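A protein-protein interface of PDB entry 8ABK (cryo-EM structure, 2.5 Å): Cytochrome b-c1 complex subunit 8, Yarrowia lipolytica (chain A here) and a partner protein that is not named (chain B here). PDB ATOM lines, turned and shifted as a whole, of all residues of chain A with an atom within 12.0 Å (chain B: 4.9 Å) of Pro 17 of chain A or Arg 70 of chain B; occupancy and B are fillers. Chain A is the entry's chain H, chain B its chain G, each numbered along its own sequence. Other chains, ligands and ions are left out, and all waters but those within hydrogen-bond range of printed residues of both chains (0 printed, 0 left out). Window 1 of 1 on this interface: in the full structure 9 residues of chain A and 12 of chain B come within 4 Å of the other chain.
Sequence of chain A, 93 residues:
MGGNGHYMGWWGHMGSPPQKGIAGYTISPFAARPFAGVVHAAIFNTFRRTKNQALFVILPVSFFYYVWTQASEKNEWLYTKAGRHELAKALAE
NH1 of Arg 70 of chain B is in salt-bridge range of OE1 of Glu 50 of chain B.
NE2 of Gln 19 of chain A is in hydrogen-bond range of OG of Ser 16 of chain A, at 3.0 Å.
Pro 17 of chain A touches Ser 67 of chain B (CB to OG, 3.9 Å).
Arg 70 of chain B touches Pro 17 of chain A.
Pro 17 of chain A touches Val 71 of chain B (CB to CG2, 3.6 Å).
Pro 18 of chain A touches Tyr 68 of chain B.
CG1 of Val 71 of chain B touches CG of Gln 19 of chain A (3.8 Å).
Lys 20 of chain A touches Tyr 68 of chain B (CB to CE1, 3.5 Å).
Ile 22 of chain A touches Tyr 72 of chain B.
Pro 17 of chain A touches just these residues of chain B: Ser 67 (3.9 Å), Arg 70 (3.97 Å) and Val 71 (3.6 Å).
Of the printed residues of chain A, Arg 70 of chain B touches Pro 17.
No residue of chain A comes within 4 Å of Asp 46 of chain B.
No residue of chain A comes within 4 Å of Glu 50 of chain B.
No residue of chain A comes within 4 Å of Leu 59 of chain B.
Of chain A, only Pro 17 (3.9 Å) comes within 4 Å of Ser 67 of chain B.
No residue of chain A comes within 4 Å of Asp 69 of chain B.
Printed residues of chain A within 4 Å of Val 71 of chain B: Pro 17 (3.6 Å) and Gln 19 (3.8 Å).
No residue of chain A comes within 4 Å of Leu 74 of chain B.
Of the printed residues of chain A, Tyr 68 of chain B touches Pro 18 (3.4 Å) and Lys 20 (3.5 Å).
Of the printed residues of chain B, Pro 18 of chain A touches Tyr 68.
Of the printed residues of chain B, Lys 20 of chain A touches Tyr 68.
Printed residues of chain B within 4 Å of Gln 19 of chain A: Val 71.
His 13 of chain A touches none of the printed residues of chain B.
The nearest residue of chain A that does not touch Arg 70 of chain B is Ile 22 of chain A (7.2 Å).
The nearest printed residue of chain B that does not touch Ile 22 of chain A is Val 71 of chain B (4.1 Å).
Of the 14 printed residues of chain B, 5 touch a printed residue of chain A.
Printed residues of chain B that touch a printed residue of chain A: Ser 67, Tyr 68, Arg 70, Val 71 and Tyr 72.
Of the 15 printed residues of chain A, 5 touch a printed residue of chain B.
Printed residues of chain A that touch a printed residue of chain B: Pro 17, Pro 18, Gln 19, Lys 20 and Ile 22.
Among the printed residues, 7 pairs touch across the chains.
Among the printed residues, no Asp or Glu carboxylate lies within 4 Å of a Lys or Arg side-chain nitrogen of the other chain.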
ATOM      1  N   TYR A   7      13.655   4.593 -12.639  1.00  0.00           N
ATOM      2  CA  TYR A   7      14.367   3.874 -13.795  1.00  0.00           C
ATOM      3  C   TYR A   7      15.517   4.669 -14.402  1.00  0.00           C
ATOM      4  O   TYR A   7      16.191   4.188 -15.315  1.00  0.00           O
ATOM      5  CB  TYR A   7      13.416   3.471 -14.923  1.00  0.00           C
ATOM      6  CG  TYR A   7      12.506   2.369 -14.476  1.00  0.00           C
ATOM      7  CD1 TYR A   7      13.008   1.112 -14.186  1.00  0.00           C
ATOM      8  CD2 TYR A   7      11.155   2.604 -14.250  1.00  0.00           C
ATOM      9  CE1 TYR A   7      12.185   0.101 -13.715  1.00  0.00           C
ATOM     10  CE2 TYR A   7      10.322   1.607 -13.772  1.00  0.00           C
ATOM     11  CZ  TYR A   7      10.841   0.351 -13.502  1.00  0.00           C
ATOM     12  OH  TYR A   7      10.019  -0.641 -13.047  1.00  0.00           O
ATOM     13  N   MET A   8      15.733   5.892 -13.940  1.00  0.00           N
ATOM     14  CA  MET A   8      16.969   6.536 -14.327  1.00  0.00           C
ATOM     15  C   MET A   8      17.558   7.143 -13.068  1.00  0.00           C
ATOM     16  O   MET A   8      16.811   7.691 -12.266  1.00  0.00           O
ATOM     17  CB  MET A   8      16.697   7.618 -15.372  1.00  0.00           C
ATOM     18  CG  MET A   8      17.936   8.402 -15.727  1.00  0.00           C
ATOM     19  SD  MET A   8      17.640   9.729 -16.924  1.00  0.00           S
ATOM     20  CE  MET A   8      16.949  11.000 -15.861  1.00  0.00           C
ATOM     21  N   GLY A   9      18.879   7.042 -12.892  1.00  0.00           N
ATOM     22  CA  GLY A   9      19.471   7.652 -11.726  1.00  0.00           C
ATOM     23  C   GLY A   9      20.043   9.005 -12.106  1.00  0.00           C
ATOM     24  O   GLY A   9      19.352   9.840 -12.691  1.00  0.00           O
ATOM     25  N   TRP A  10      21.319   9.197 -11.782  1.00  0.00           N
ATOM     26  CA  TRP A  10      21.998  10.433 -12.128  1.00  0.00           C
ATOM     27  C   TRP A  10      23.467  10.120 -12.378  1.00  0.00           C
ATOM     28  O   TRP A  10      23.874   8.979 -12.204  1.00  0.00           O
ATOM     29  CB  TRP A  10      21.811  11.456 -11.013  1.00  0.00           C
ATOM     30  CG  TRP A  10      21.946  12.858 -11.517  1.00  0.00           C
ATOM     31  CD1 TRP A  10      22.986  13.723 -11.311  1.00  0.00           C
ATOM     32  CD2 TRP A  10      21.018  13.537 -12.379  1.00  0.00           C
ATOM     33  NE1 TRP A  10      22.753  14.911 -11.960  1.00  0.00           N
ATOM     34  CE2 TRP A  10      21.550  14.832 -12.615  1.00  0.00           C
ATOM     35  CE3 TRP A  10      19.786  13.183 -12.950  1.00  0.00           C
ATOM     36  CZ2 TRP A  10      20.885  15.772 -13.405  1.00  0.00           C
ATOM     37  CZ3 TRP A  10      19.123  14.117 -13.717  1.00  0.00           C
ATOM     38  CH2 TRP A  10      19.670  15.392 -13.940  1.00  0.00           C
ATOM     39  N   GLY A  12      27.106   9.087 -12.194  1.00  0.00           N
ATOM     40  CA  GLY A  12      27.709   8.304 -11.132  1.00  0.00           C
ATOM     41  C   GLY A  12      26.879   7.079 -10.751  1.00  0.00           C
ATOM     42  O   GLY A  12      27.445   6.086 -10.307  1.00  0.00           O
ATOM     43  N   HIS A  13      25.554   7.131 -10.921  1.00  0.00           N
ATOM     44  CA  HIS A  13      24.697   6.018 -10.547  1.00  0.00           C
ATOM     45  C   HIS A  13      23.500   6.035 -11.484  1.00  0.00           C
ATOM     46  O   HIS A  13      22.352   6.120 -11.055  1.00  0.00           O
ATOM     47  CB  HIS A  13      24.316   6.088  -9.055  1.00  0.00           C
ATOM     48  CG  HIS A  13      23.655   7.369  -8.658  1.00  0.00           C
ATOM     49  ND1 HIS A  13      24.372   8.530  -8.462  1.00  0.00           N
ATOM     50  CD2 HIS A  13      22.352   7.689  -8.459  1.00  0.00           C
ATOM     51  CE1 HIS A  13      23.545   9.511  -8.153  1.00  0.00           C
ATOM     52  NE2 HIS A  13      22.294   9.022  -8.151  1.00  0.00           N
ATOM     53  N   MET A  14      23.785   5.981 -12.782  1.00  0.00           N
ATOM     54  CA  MET A  14      22.738   6.161 -13.766  1.00  0.00           C
ATOM     55  C   MET A  14      21.765   4.978 -13.777  1.00  0.00           C
ATOM     56  O   MET A  14      20.616   5.144 -14.166  1.00  0.00           O
ATOM     57  CB  MET A  14      23.340   6.360 -15.157  1.00  0.00           C
ATOM     58  CG  MET A  14      22.371   6.954 -16.159  1.00  0.00           C
ATOM     59  SD  MET A  14      22.020   8.664 -15.713  1.00  0.00           S
ATOM     60  CE  MET A  14      23.656   9.373 -15.935  1.00  0.00           C
ATOM     61  N   GLY A  15      22.198   3.798 -13.321  1.00  0.00           N
ATOM     62  CA  GLY A  15      21.334   2.627 -13.319  1.00  0.00           C
ATOM     63  C   GLY A  15      21.720   1.612 -14.393  1.00  0.00           C
ATOM     64  O   GLY A  15      20.980   0.660 -14.640  1.00  0.00           O
ATOM     65  N   SER A  16      22.889   1.814 -15.014  1.00  0.00           N
ATOM     66  CA  SER A  16      23.460   0.875 -15.964  1.00  0.00           C
ATOM     67  C   SER A  16      23.828  -0.392 -15.207  1.00  0.00           C
ATOM     68  O   SER A  16      24.242  -0.316 -14.054  1.00  0.00           O
ATOM     69  CB  SER A  16      24.671   1.488 -16.643  1.00  0.00           C
ATOM     70  OG  SER A  16      25.441   0.534 -17.361  1.00  0.00           O
ATOM     71  N   PRO A  17      23.704  -1.588 -15.816  1.00  0.00           N
ATOM     72  CA  PRO A  17      24.370  -2.768 -15.265  1.00  0.00           C
ATOM     73  C   PRO A  17      25.853  -2.431 -15.218  1.00  0.00           C
ATOM     74  O   PRO A  17      26.302  -1.556 -15.951  1.00  0.00           O
ATOM     75  CB  PRO A  17      24.187  -3.812 -16.363  1.00  0.00           C
ATOM     76  CG  PRO A  17      22.948  -3.362 -17.095  1.00  0.00           C
ATOM     77  CD  PRO A  17      22.976  -1.852 -17.068  1.00  0.00           C
ATOM     78  N   PRO A  18      26.660  -3.096 -14.368  1.00  0.00           N
ATOM     79  CA  PRO A  18      28.096  -2.825 -14.306  1.00  0.00           C
ATOM     80  C   PRO A  18      28.745  -2.940 -15.677  1.00  0.00           C
ATOM     81  O   PRO A  18      28.488  -3.881 -16.421  1.00  0.00           O
ATOM     82  CB  PRO A  18      28.608  -3.984 -13.460  1.00  0.00           C
ATOM     83  CG  PRO A  18      27.451  -4.280 -12.551  1.00  0.00           C
ATOM     84  CD  PRO A  18      26.235  -4.147 -13.434  1.00  0.00           C
ATOM     85  N   GLN A  19      29.578  -1.959 -16.000  1.00  0.00           N
ATOM     86  CA  GLN A  19      30.272  -1.979 -17.271  1.00  0.00           C
ATOM     87  C   GLN A  19      31.709  -2.391 -17.013  1.00  0.00           C
ATOM     88  O   GLN A  19      32.330  -1.912 -16.066  1.00  0.00           O
ATOM     89  CB  GLN A  19      30.236  -0.597 -17.912  1.00  0.00           C
ATOM     90  CG  GLN A  19      28.829  -0.043 -18.020  1.00  0.00           C
ATOM     91  CD  GLN A  19      28.722   1.070 -19.031  1.00  0.00           C
ATOM     92  OE1 GLN A  19      29.707   1.500 -19.632  1.00  0.00           O
ATOM     93  NE2 GLN A  19      27.507   1.563 -19.211  1.00  0.00           N
ATOM     94  N   LYS A  20      32.206  -3.301 -17.846  1.00  0.00           N
ATOM     95  CA  LYS A  20      33.594  -3.695 -17.763  1.00  0.00           C
ATOM     96  C   LYS A  20      34.030  -4.195 -19.130  1.00  0.00           C
ATOM     97  O   LYS A  20      33.258  -4.848 -19.813  1.00  0.00           O
ATOM     98  CB  LYS A  20      33.730  -4.802 -16.722  1.00  0.00           C
ATOM     99  CG  LYS A  20      35.157  -5.084 -16.312  1.00  0.00           C
ATOM    100  CD  LYS A  20      35.196  -5.952 -15.090  1.00  0.00           C
ATOM    101  CE  LYS A  20      36.594  -6.418 -14.757  1.00  0.00           C
ATOM    102  NZ  LYS A  20      36.562  -7.437 -13.683  1.00  0.00           N
ATOM    103  N   GLY A  21      35.263  -3.868 -19.518  1.00  0.00           N
ATOM    104  CA  GLY A  21      35.869  -4.467 -20.693  1.00  0.00           C
ATOM    105  C   GLY A  21      35.686  -3.652 -21.970  1.00  0.00           C
ATOM    106  O   GLY A  21      36.162  -4.080 -23.020  1.00  0.00           O
ATOM    107  N   ILE A  22      35.010  -2.497 -21.893  1.00  0.00           N
ATOM    108  CA  ILE A  22      34.870  -1.647 -23.066  1.00  0.00           C
ATOM    109  C   ILE A  22      35.855  -0.489 -22.965  1.00  0.00           C
ATOM    110  O   ILE A  22      35.821   0.262 -22.002  1.00  0.00           O
ATOM    111  CB  ILE A  22      33.431  -1.118 -23.186  1.00  0.00           C
ATOM    112  CG1 ILE A  22      32.408  -2.250 -23.177  1.00  0.00           C
ATOM    113  CG2 ILE A  22      33.269  -0.217 -24.405  1.00  0.00           C
ATOM    114  CD1 ILE A  22      31.014  -1.778 -22.882  1.00  0.00           C
ATOM    115  N   ASP B  46      17.810  -8.497 -26.584  1.00  0.00           N
ATOM    116  CA  ASP B  46      18.249  -7.161 -26.200  1.00  0.00           C
ATOM    117  C   ASP B  46      17.130  -6.132 -26.338  1.00  0.00           C
ATOM    118  O   ASP B  46      17.204  -5.072 -25.727  1.00  0.00           O
ATOM    119  CB  ASP B  46      19.423  -6.670 -27.037  1.00  0.00           C
ATOM    120  CG  ASP B  46      20.633  -7.576 -26.962  1.00  0.00           C
ATOM    121  OD1 ASP B  46      20.832  -8.216 -25.905  1.00  0.00           O
ATOM    122  OD2 ASP B  46      21.370  -7.641 -27.960  1.00  0.00           O
ATOM    123  N   GLU B  50      12.858  -3.248 -20.521  1.00  0.00           N
ATOM    124  CA  GLU B  50      13.397  -3.697 -19.249  1.00  0.00           C
ATOM    125  C   GLU B  50      12.945  -2.868 -18.053  1.00  0.00           C
ATOM    126  O   GLU B  50      13.274  -3.223 -16.923  1.00  0.00           O
ATOM    127  CB  GLU B  50      14.912  -3.832 -19.258  1.00  0.00           C
ATOM    128  CG  GLU B  50      15.623  -2.778 -20.031  1.00  0.00           C
ATOM    129  CD  GLU B  50      16.320  -1.794 -19.123  1.00  0.00           C
ATOM    130  OE1 GLU B  50      17.262  -2.191 -18.403  1.00  0.00           O
ATOM    131  OE2 GLU B  50      15.923  -0.626 -19.132  1.00  0.00           O
ATOM    132  N   LEU B  59      17.325  -9.246 -15.128  1.00  0.00           N
ATOM    133  CA  LEU B  59      18.603  -8.766 -15.627  1.00  0.00           C
ATOM    134  C   LEU B  59      19.682  -8.897 -14.558  1.00  0.00           C
ATOM    135  O   LEU B  59      20.831  -9.164 -14.890  1.00  0.00           O
ATOM    136  CB  LEU B  59      18.481  -7.326 -16.131  1.00  0.00           C
ATOM    137  CG  LEU B  59      17.808  -7.155 -17.492  1.00  0.00           C
ATOM    138  CD1 LEU B  59      17.502  -5.691 -17.746  1.00  0.00           C
ATOM    139  CD2 LEU B  59      18.631  -7.762 -18.625  1.00  0.00           C
ATOM    140  N   LEU B  62      21.278 -12.317 -14.598  1.00  0.00           N
ATOM    141  CA  LEU B  62      22.144 -12.752 -15.684  1.00  0.00           C
ATOM    142  C   LEU B  62      23.530 -13.077 -15.138  1.00  0.00           C
ATOM    143  O   LEU B  62      24.051 -12.376 -14.274  1.00  0.00           O
ATOM    144  CB  LEU B  62      22.275 -11.634 -16.715  1.00  0.00           C
ATOM    145  CG  LEU B  62      21.175 -11.534 -17.763  1.00  0.00           C
ATOM    146  CD1 LEU B  62      21.547 -10.457 -18.773  1.00  0.00           C
ATOM    147  CD2 LEU B  62      20.977 -12.873 -18.458  1.00  0.00           C
ATOM    148  N   GLU B  66      27.412 -12.650 -19.516  1.00  0.00           N
ATOM    149  CA  GLU B  66      26.273 -12.320 -20.359  1.00  0.00           C
ATOM    150  C   GLU B  66      25.880 -10.864 -20.130  1.00  0.00           C
ATOM    151  O   GLU B  66      25.516 -10.164 -21.064  1.00  0.00           O
ATOM    152  CB  GLU B  66      25.076 -13.212 -20.039  1.00  0.00           C
ATOM    153  CG  GLU B  66      25.298 -14.673 -20.380  1.00  0.00           C
ATOM    154  CD  GLU B  66      24.847 -15.084 -21.773  1.00  0.00           C
ATOM    155  OE1 GLU B  66      24.524 -16.278 -21.952  1.00  0.00           O
ATOM    156  OE2 GLU B  66      24.776 -14.215 -22.681  1.00  0.00           O
ATOM    157  N   SER B  67      25.950 -10.431 -18.876  1.00  0.00           N
ATOM    158  CA  SER B  67      25.579  -9.075 -18.547  1.00  0.00           C
ATOM    159  C   SER B  67      26.543  -8.086 -19.197  1.00  0.00           C
ATOM    160  O   SER B  67      26.088  -7.100 -19.763  1.00  0.00           O
ATOM    161  CB  SER B  67      25.503  -8.906 -17.069  1.00  0.00           C
ATOM    162  OG  SER B  67      25.206  -7.559 -16.725  1.00  0.00           O
ATOM    163  N   TYR B  68      27.853  -8.352 -19.133  1.00  0.00           N
ATOM    164  CA  TYR B  68      28.827  -7.435 -19.700  1.00  0.00           C
ATOM    165  C   TYR B  68      28.685  -7.396 -21.208  1.00  0.00           C
ATOM    166  O   TYR B  68      28.837  -6.349 -21.806  1.00  0.00           O
ATOM    167  CB  TYR B  68      30.263  -7.862 -19.422  1.00  0.00           C
ATOM    168  CG  TYR B  68      30.656  -7.707 -17.983  1.00  0.00           C
ATOM    169  CD1 TYR B  68      30.376  -6.539 -17.288  1.00  0.00           C
ATOM    170  CD2 TYR B  68      31.294  -8.738 -17.309  1.00  0.00           C
ATOM    171  CE1 TYR B  68      30.737  -6.393 -15.956  1.00  0.00           C
ATOM    172  CE2 TYR B  68      31.666  -8.607 -15.981  1.00  0.00           C
ATOM    173  CZ  TYR B  68      31.394  -7.427 -15.307  1.00  0.00           C
ATOM    174  OH  TYR B  68      31.755  -7.297 -13.995  1.00  0.00           O
ATOM    175  N   ASP B  69      28.363  -8.527 -21.824  1.00  0.00           N
ATOM    176  CA  ASP B  69      28.256  -8.520 -23.268  1.00  0.00           C
ATOM    177  C   ASP B  69      26.999  -7.789 -23.724  1.00  0.00           C
ATOM    178  O   ASP B  69      26.976  -7.205 -24.803  1.00  0.00           O
ATOM    179  CB  ASP B  69      28.137  -9.936 -23.788  1.00  0.00           C
ATOM    180  CG  ASP B  69      29.397 -10.761 -23.652  1.00  0.00           C
ATOM    181  OD1 ASP B  69      30.458 -10.203 -23.294  1.00  0.00           O
ATOM    182  OD2 ASP B  69      29.315 -11.974 -23.940  1.00  0.00           O
ATOM    183  N   ARG B  70      25.927  -7.877 -22.936  1.00  0.00           N
ATOM    184  CA  ARG B  70      24.717  -7.166 -23.292  1.00  0.00           C
ATOM    185  C   ARG B  70      24.994  -5.665 -23.232  1.00  0.00           C
ATOM    186  O   ARG B  70      24.605  -4.930 -24.129  1.00  0.00           O
ATOM    187  CB  ARG B  70      23.591  -7.582 -22.350  1.00  0.00           C
ATOM    188  CG  ARG B  70      22.309  -6.784 -22.530  1.00  0.00           C
ATOM    189  CD  ARG B  70      21.158  -7.276 -21.669  1.00  0.00           C
ATOM    190  NE  ARG B  70      20.012  -6.370 -21.682  1.00  0.00           N
ATOM    191  CZ  ARG B  70      19.914  -5.270 -20.931  1.00  0.00           C
ATOM    192  NH1 ARG B  70      18.828  -4.519 -20.997  1.00  0.00           N
ATOM    193  NH2 ARG B  70      20.884  -4.940 -20.093  1.00  0.00           N
ATOM    194  N   VAL B  71      25.696  -5.217 -22.194  1.00  0.00           N
ATOM    195  CA  VAL B  71      26.001  -3.806 -22.094  1.00  0.00           C
ATOM    196  C   VAL B  71      26.764  -3.372 -23.343  1.00  0.00           C
ATOM    197  O   VAL B  71      26.463  -2.334 -23.919  1.00  0.00           O
ATOM    198  CB  VAL B  71      26.781  -3.496 -20.806  1.00  0.00           C
ATOM    199  CG1 VAL B  71      27.458  -2.136 -20.850  1.00  0.00           C
ATOM    200  CG2 VAL B  71      25.884  -3.589 -19.586  1.00  0.00           C
ATOM    201  N   TYR B  72      27.715  -4.182 -23.794  1.00  0.00           N
ATOM    202  CA  TYR B  72      28.456  -3.782 -24.975  1.00  0.00           C
ATOM    203  C   TYR B  72      27.579  -3.729 -26.229  1.00  0.00           C
ATOM    204  O   TYR B  72      27.697  -2.793 -27.017  1.00  0.00           O
ATOM    205  CB  TYR B  72      29.682  -4.661 -25.189  1.00  0.00           C
ATOM    206  CG  TYR B  72      30.371  -4.360 -26.494  1.00  0.00           C
ATOM    207  CD1 TYR B  72      31.000  -3.136 -26.683  1.00  0.00           C
ATOM    208  CD2 TYR B  72      30.346  -5.258 -27.556  1.00  0.00           C
ATOM    209  CE1 TYR B  72      31.610  -2.814 -27.885  1.00  0.00           C
ATOM    210  CE2 TYR B  72      30.973  -4.963 -28.760  1.00  0.00           C
ATOM    211  CZ  TYR B  72      31.613  -3.739 -28.914  1.00  0.00           C
ATOM    212  OH  TYR B  72      32.245  -3.397 -30.074  1.00  0.00           O
ATOM    213  N   ARG B  73      26.699  -4.713 -26.426  1.00  0.00           N
ATOM    214  CA  ARG B  73      25.827  -4.667 -27.587  1.00  0.00           C
ATOM    215  C   ARG B  73      24.914  -3.441 -27.556  1.00  0.00           C
ATOM    216  O   ARG B  73      24.663  -2.854 -28.601  1.00  0.00           O
ATOM    217  CB  ARG B  73      24.995  -5.941 -27.702  1.00  0.00           C
ATOM    218  CG  ARG B  73      25.789  -7.162 -28.139  1.00  0.00           C
ATOM    219  CD  ARG B  73      24.875  -8.312 -28.511  1.00  0.00           C
ATOM    220  NE  ARG B  73      23.925  -8.608 -27.454  1.00  0.00           N
ATOM    221  CZ  ARG B  73      24.145  -9.378 -26.388  1.00  0.00           C
ATOM    222  NH1 ARG B  73      23.176  -9.522 -25.506  1.00  0.00           N
ATOM    223  NH2 ARG B  73      25.309  -9.976 -26.198  1.00  0.00           N
ATOM    224  N   LEU B  74      24.435  -3.032 -26.375  1.00  0.00           N
ATOM    225  CA  LEU B  74      23.565  -1.865 -26.312  1.00  0.00           C
ATOM    226  C   LEU B  74      24.344  -0.601 -26.657  1.00  0.00           C
ATOM    227  O   LEU B  74      23.840   0.249 -27.387  1.00  0.00           O
ATOM    228  CB  LEU B  74      22.947  -1.738 -24.921  1.00  0.00           C
ATOM    229  CG  LEU B  74      22.039  -2.879 -24.475  1.00  0.00           C
ATOM    230  CD1 LEU B  74      21.487  -2.579 -23.095  1.00  0.00           C
ATOM    231  CD2 LEU B  74      20.907  -3.142 -25.465  1.00  0.00           C
ATOM    232  N   TYR B 101      19.295 -15.638 -24.468  1.00  0.00           N
ATOM    233  CA  TYR B 101      20.052 -15.702 -23.230  1.00  0.00           C
ATOM    234  C   TYR B 101      19.164 -15.261 -22.061  1.00  0.00           C
ATOM    235  O   TYR B 101      19.411 -15.650 -20.933  1.00  0.00           O
ATOM    236  CB  TYR B 101      21.355 -14.896 -23.348  1.00  0.00           C
ATOM    237  CG  TYR B 101      21.079 -13.420 -23.462  1.00  0.00           C
ATOM    238  CD1 TYR B 101      20.857 -12.641 -22.333  1.00  0.00           C
ATOM    239  CD2 TYR B 101      20.904 -12.825 -24.704  1.00  0.00           C
ATOM    240  CE1 TYR B 101      20.509 -11.299 -22.436  1.00  0.00           C
ATOM    241  CE2 TYR B 101      20.575 -11.482 -24.826  1.00  0.00           C
ATOM    242  CZ  TYR B 101      20.373 -10.714 -23.688  1.00  0.00           C
ATOM    243  OH  TYR B 101      20.010  -9.400 -23.828  1.00  0.00           O
